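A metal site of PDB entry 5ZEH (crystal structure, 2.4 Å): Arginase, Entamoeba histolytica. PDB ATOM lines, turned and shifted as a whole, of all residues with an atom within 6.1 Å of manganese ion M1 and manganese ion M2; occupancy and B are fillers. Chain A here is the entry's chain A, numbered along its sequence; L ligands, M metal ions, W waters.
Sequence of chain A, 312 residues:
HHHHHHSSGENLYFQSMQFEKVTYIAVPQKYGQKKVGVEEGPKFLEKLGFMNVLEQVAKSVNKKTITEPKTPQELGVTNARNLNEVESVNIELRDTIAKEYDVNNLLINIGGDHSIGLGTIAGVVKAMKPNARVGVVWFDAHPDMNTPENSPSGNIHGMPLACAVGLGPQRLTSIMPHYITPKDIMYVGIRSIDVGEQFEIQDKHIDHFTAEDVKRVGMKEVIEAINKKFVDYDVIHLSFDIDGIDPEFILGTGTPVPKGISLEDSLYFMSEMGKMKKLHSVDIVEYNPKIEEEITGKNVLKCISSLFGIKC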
ATOM      1  N   HIS A 114     -25.199   2.311  -6.298  1.00  0.00           N
ATOM      2  CA  HIS A 114     -25.181   3.754  -6.499  1.00  0.00           C
ATOM      3  C   HIS A 114     -24.098   4.250  -7.480  1.00  0.00           C
ATOM      4  O   HIS A 114     -23.988   5.444  -7.695  1.00  0.00           O
ATOM      5  CB  HIS A 114     -25.056   4.496  -5.161  1.00  0.00           C
ATOM      6  CG  HIS A 114     -25.860   5.759  -5.102  1.00  0.00           C
ATOM      7  ND1 HIS A 114     -26.215   6.348  -3.906  1.00  0.00           N
ATOM      8  CD2 HIS A 114     -26.417   6.517  -6.070  1.00  0.00           C
ATOM      9  CE1 HIS A 114     -26.934   7.423  -4.142  1.00  0.00           C
ATOM     10  NE2 HIS A 114     -27.077   7.547  -5.452  1.00  0.00           N
ATOM     11  N   TRP A 138     -28.873  14.369  -2.734  1.00  0.00           N
ATOM     12  CA  TRP A 138     -28.227  13.072  -2.618  1.00  0.00           C
ATOM     13  C   TRP A 138     -28.479  12.507  -1.220  1.00  0.00           C
ATOM     14  O   TRP A 138     -27.699  12.733  -0.293  1.00  0.00           O
ATOM     15  CB  TRP A 138     -26.751  13.211  -2.932  1.00  0.00           C
ATOM     16  CG  TRP A 138     -26.040  11.944  -3.131  1.00  0.00           C
ATOM     17  CD1 TRP A 138     -25.505  11.162  -2.165  1.00  0.00           C
ATOM     18  CD2 TRP A 138     -25.718  11.312  -4.380  1.00  0.00           C
ATOM     19  NE1 TRP A 138     -24.884  10.065  -2.728  1.00  0.00           N
ATOM     20  CE2 TRP A 138     -25.006  10.142  -4.086  1.00  0.00           C
ATOM     21  CE3 TRP A 138     -25.974  11.624  -5.718  1.00  0.00           C
ATOM     22  CZ2 TRP A 138     -24.535   9.266  -5.080  1.00  0.00           C
ATOM     23  CZ3 TRP A 138     -25.510  10.741  -6.708  1.00  0.00           C
ATOM     24  CH2 TRP A 138     -24.802   9.590  -6.389  1.00  0.00           C
ATOM     25  N   PHE A 139     -29.593  11.790  -1.111  1.00  0.00           N
ATOM     26  CA  PHE A 139     -30.075  11.185   0.135  1.00  0.00           C
ATOM     27  C   PHE A 139     -29.379   9.843   0.288  1.00  0.00           C
ATOM     28  O   PHE A 139     -29.596   8.943  -0.530  1.00  0.00           O
ATOM     29  CB  PHE A 139     -31.600  11.011   0.035  1.00  0.00           C
ATOM     30  CG  PHE A 139     -32.250  10.430   1.246  1.00  0.00           C
ATOM     31  CD1 PHE A 139     -32.270   9.047   1.442  1.00  0.00           C
ATOM     32  CD2 PHE A 139     -32.897  11.242   2.170  1.00  0.00           C
ATOM     33  CE1 PHE A 139     -32.888   8.507   2.540  1.00  0.00           C
ATOM     34  CE2 PHE A 139     -33.525  10.702   3.277  1.00  0.00           C
ATOM     35  CZ  PHE A 139     -33.522   9.323   3.467  1.00  0.00           C
ATOM     36  N   ASP A 140     -28.543   9.713   1.323  1.00  0.00           N
ATOM     37  CA  ASP A 140     -27.597   8.594   1.420  1.00  0.00           C
ATOM     38  C   ASP A 140     -26.907   8.571   2.793  1.00  0.00           C
ATOM     39  O   ASP A 140     -26.810   9.601   3.443  1.00  0.00           O
ATOM     40  CB  ASP A 140     -26.538   8.731   0.298  1.00  0.00           C
ATOM     41  CG  ASP A 140     -25.863   7.423  -0.062  1.00  0.00           C
ATOM     42  OD1 ASP A 140     -25.560   6.605   0.866  1.00  0.00           O
ATOM     43  OD2 ASP A 140     -25.604   7.212  -1.266  1.00  0.00           O
ATOM     44  N   ALA A 141     -26.450   7.396   3.250  1.00  0.00           N
ATOM     45  CA  ALA A 141     -25.547   7.314   4.407  1.00  0.00           C
ATOM     46  C   ALA A 141     -24.115   7.780   4.061  1.00  0.00           C
ATOM     47  O   ALA A 141     -23.350   8.245   4.929  1.00  0.00           O
ATOM     48  CB  ALA A 141     -25.504   5.911   4.972  1.00  0.00           C
ATOM     49  N   HIS A 142     -23.772   7.620   2.798  1.00  0.00           N
ATOM     50  CA  HIS A 142     -22.481   7.940   2.267  1.00  0.00           C
ATOM     51  C   HIS A 142     -22.434   9.083   1.294  1.00  0.00           C
ATOM     52  O   HIS A 142     -23.338   9.244   0.514  1.00  0.00           O
ATOM     53  CB  HIS A 142     -22.036   6.755   1.458  1.00  0.00           C
ATOM     54  CG  HIS A 142     -22.198   5.451   2.161  1.00  0.00           C
ATOM     55  ND1 HIS A 142     -23.275   4.629   1.963  1.00  0.00           N
ATOM     56  CD2 HIS A 142     -21.401   4.820   3.048  1.00  0.00           C
ATOM     57  CE1 HIS A 142     -23.135   3.545   2.699  1.00  0.00           C
ATOM     58  NE2 HIS A 142     -22.004   3.636   3.356  1.00  0.00           N
ATOM     59  N   ASP A 144     -20.330   9.284  -1.212  1.00  0.00           N
ATOM     60  CA  ASP A 144     -19.911   8.733  -2.496  1.00  0.00           C
ATOM     61  C   ASP A 144     -19.003   9.684  -3.274  1.00  0.00           C
ATOM     62  O   ASP A 144     -19.193   9.918  -4.475  1.00  0.00           O
ATOM     63  CB  ASP A 144     -21.116   8.337  -3.341  1.00  0.00           C
ATOM     64  CG  ASP A 144     -21.937   7.252  -2.702  1.00  0.00           C
ATOM     65  OD1 ASP A 144     -21.414   6.468  -1.894  1.00  0.00           O
ATOM     66  OD2 ASP A 144     -23.132   7.167  -3.033  1.00  0.00           O
ATOM     67  N   HIS A 157     -19.210   2.279  -6.602  1.00  0.00           N
ATOM     68  CA  HIS A 157     -20.429   2.895  -6.031  1.00  0.00           C
ATOM     69  C   HIS A 157     -20.169   3.923  -4.916  1.00  0.00           C
ATOM     70  O   HIS A 157     -21.100   4.631  -4.508  1.00  0.00           O
ATOM     71  CB  HIS A 157     -21.457   1.828  -5.615  1.00  0.00           C
ATOM     72  CG  HIS A 157     -21.236   1.228  -4.258  1.00  0.00           C
ATOM     73  ND1 HIS A 157     -22.263   0.678  -3.515  1.00  0.00           N
ATOM     74  CD2 HIS A 157     -20.121   1.082  -3.513  1.00  0.00           C
ATOM     75  CE1 HIS A 157     -21.797   0.211  -2.380  1.00  0.00           C
ATOM     76  NE2 HIS A 157     -20.490   0.454  -2.351  1.00  0.00           N
ATOM     77  N   PRO A 160     -19.127   7.691  -7.594  1.00  0.00           N
ATOM     78  CA  PRO A 160     -19.949   8.409  -8.584  1.00  0.00           C
ATOM     79  C   PRO A 160     -20.112   9.901  -8.504  1.00  0.00           C
ATOM     80  O   PRO A 160     -20.094  10.523  -9.513  1.00  0.00           O
ATOM     81  CB  PRO A 160     -21.326   7.782  -8.398  1.00  0.00           C
ATOM     82  CG  PRO A 160     -21.325   7.369  -6.986  1.00  0.00           C
ATOM     83  CD  PRO A 160     -19.971   6.753  -6.842  1.00  0.00           C
ATOM     84  N   ASP A 241     -30.648   6.821  -2.043  1.00  0.00           N
ATOM     85  CA  ASP A 241     -29.994   5.586  -1.590  1.00  0.00           C
ATOM     86  C   ASP A 241     -30.890   5.171  -0.433  1.00  0.00           C
ATOM     87  O   ASP A 241     -31.127   5.953   0.454  1.00  0.00           O
ATOM     88  CB  ASP A 241     -28.594   5.916  -1.030  1.00  0.00           C
ATOM     89  CG  ASP A 241     -27.616   4.719  -0.988  1.00  0.00           C
ATOM     90  OD1 ASP A 241     -28.072   3.563  -0.722  1.00  0.00           O
ATOM     91  OD2 ASP A 241     -26.411   4.900  -1.138  1.00  0.00           O
ATOM     92  N   ASP A 243     -30.228   3.176   1.924  1.00  0.00           N
ATOM     93  CA  ASP A 243     -29.453   3.040   3.166  1.00  0.00           C
ATOM     94  C   ASP A 243     -29.211   4.365   3.894  1.00  0.00           C
ATOM     95  O   ASP A 243     -28.670   4.363   4.991  1.00  0.00           O
ATOM     96  CB  ASP A 243     -28.193   2.185   2.994  1.00  0.00           C
ATOM     97  CG  ASP A 243     -27.016   2.933   2.432  1.00  0.00           C
ATOM     98  OD1 ASP A 243     -26.536   3.924   3.039  1.00  0.00           O
ATOM     99  OD2 ASP A 243     -26.530   2.482   1.358  1.00  0.00           O
ATOM    100  N   GLY A 244     -29.631   5.479   3.313  1.00  0.00           N
ATOM    101  CA  GLY A 244     -29.793   6.713   4.060  1.00  0.00           C
ATOM    102  C   GLY A 244     -30.815   6.563   5.171  1.00  0.00           C
ATOM    103  O   GLY A 244     -30.750   7.281   6.178  1.00  0.00           O
ATOM    104  N   THR A 255     -24.517  -2.027   2.298  1.00  0.00           N
ATOM    105  CA  THR A 255     -23.782  -1.263   3.294  1.00  0.00           C
ATOM    106  C   THR A 255     -24.718  -0.491   4.231  1.00  0.00           C
ATOM    107  O   THR A 255     -24.795   0.730   4.168  1.00  0.00           O
ATOM    108  CB  THR A 255     -22.774  -0.305   2.622  1.00  0.00           C
ATOM    109  OG1 THR A 255     -23.473   0.678   1.833  1.00  0.00           O
ATOM    110  CG2 THR A 255     -21.800  -1.071   1.736  1.00  0.00           C
ATOM    111  N   VAL A 285     -32.056   3.523  -5.233  1.00  0.00           N
ATOM    112  CA  VAL A 285     -30.858   2.690  -5.369  1.00  0.00           C
ATOM    113  C   VAL A 285     -30.479   1.867  -4.133  1.00  0.00           C
ATOM    114  O   VAL A 285     -30.881   2.176  -3.003  1.00  0.00           O
ATOM    115  CB  VAL A 285     -29.665   3.542  -5.826  1.00  0.00           C
ATOM    116  CG1 VAL A 285     -29.883   4.097  -7.229  1.00  0.00           C
ATOM    117  CG2 VAL A 285     -29.322   4.654  -4.843  1.00  0.00           C
ATOM    118  N   GLU A 286     -29.716   0.809  -4.380  1.00  0.00           N
ATOM    119  CA  GLU A 286     -29.099  -0.064  -3.352  1.00  0.00           C
ATOM    120  C   GLU A 286     -30.078  -0.960  -2.602  1.00  0.00           C
ATOM    121  O   GLU A 286     -29.825  -1.309  -1.442  1.00  0.00           O
ATOM    122  CB  GLU A 286     -28.250   0.744  -2.320  1.00  0.00           C
ATOM    123  CG  GLU A 286     -27.042   1.509  -2.849  1.00  0.00           C
ATOM    124  CD  GLU A 286     -25.886   0.641  -3.308  1.00  0.00           C
ATOM    125  OE1 GLU A 286     -25.930  -0.609  -3.186  1.00  0.00           O
ATOM    126  OE2 GLU A 286     -24.905   1.244  -3.823  1.00  0.00           O
HETATM  127  N1  LIG L   1     -17.085   4.888   1.320  1.00  0.00           N
HETATM  128  C1  LIG L   1     -17.198   3.429   1.141  1.00  0.00           C
HETATM  129  C2  LIG L   1     -18.663   2.974   1.130  1.00  0.00           C
HETATM  130  C3  LIG L   1     -19.504   3.773   0.116  1.00  0.00           C
HETATM  131  C4  LIG L   1     -20.844   3.074  -0.079  1.00  0.00           C
HETATM  132  N2  LIG L   1     -21.675   3.772  -1.068  1.00  0.00           N
HETATM  133  C5  LIG L   1     -16.481   2.942  -0.128  1.00  0.00           C
HETATM  134  O1  LIG L   1     -16.401   1.709  -0.268  1.00  0.00           O
HETATM  135  O2  LIG L   1     -16.048   3.780  -0.942  1.00  0.00           O
HETATM  136 MN    MN M   1     -24.736   5.737  -2.281  1.00  0.00          MN
HETATM  137 MN    MN M   2     -25.360   4.670   0.869  1.00  0.00          MN
HETATM  138  O   HOH W   1     -23.333   3.521  -3.057  1.00  0.00           O
HETATM  139  O   HOH W   2     -24.375   4.028  -0.769  1.00  0.00           O
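OD1 of Asp 144 is in salt-bridge range of N2 of the ligand, 2.8 Å away.
N of His 114 lies within hydrogen-bond range of OE2 of Glu 286, 2.7 Å away.
The side-chain carboxylate (OD1) of Asp 243 sits close to the backbone NH (N) of Ala 141.
The backbone carbonyl oxygen of Phe 139 sits at hydrogen-bond distance from the backbone NH of Asp 241 (2.8 Å).
OD2 of Asp 144 sits close to NE1 of Trp 138, at 3.4 Å.
NE1 of Trp 138 sits close to OD2 of Asp 140 (3.3 Å).
Four residues have an atom within 4 Å of manganese ion M1: His 114, Asp 140, Asp 144 and Asp 241.
The nearest printed residue that does not touch manganese ion M1 is Trp 138 (4.4 Å).
Ala 141 touches manganese ion M2 (N to MN, 3.8 Å).
Of the 15 residues printed, 5 come within 4 Å of manganese ion M2.
The nearest printed residue that does not touch manganese ion M2 is Thr 255 (4.5 Å).
The side-chain carboxylate (OD2) of Asp 140 is bound to manganese ion M1.
OD2 of Asp 241 is bound to manganese ion M1.
OD2 of Asp 144 is bound to manganese ion M1.
Manganese ion M1 is bound by ND1 of His 114 (2.3 Å).
Water W2 is bound to manganese ion M1 (2.3 Å).
Slightly farther from manganese ion M1 lies water W1 (2.7 Å).
Manganese ion M2 is bound by OD1 of Asp 140.
Manganese ion M2 is bound by water W2 (2.0 Å).
OD2 of Asp 241 binds manganese ion M2 (2.3 Å).
A ring nitrogen (ND1) of His 142 is bound to manganese ion M2 (2.4 Å).
OD2 of Asp 243 binds manganese ion M2 (2.5 Å).
OD1 of Asp 243 binds manganese ion M2 (2.6 Å).
Manganese ion M2 has six donor atoms within binding distance.
Water W1 lies within hydrogen-bond range of N2 of the ligand (2.6 Å), OE2 of Glu 286 (2.9 Å) and O of His 157 (2.9 Å).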
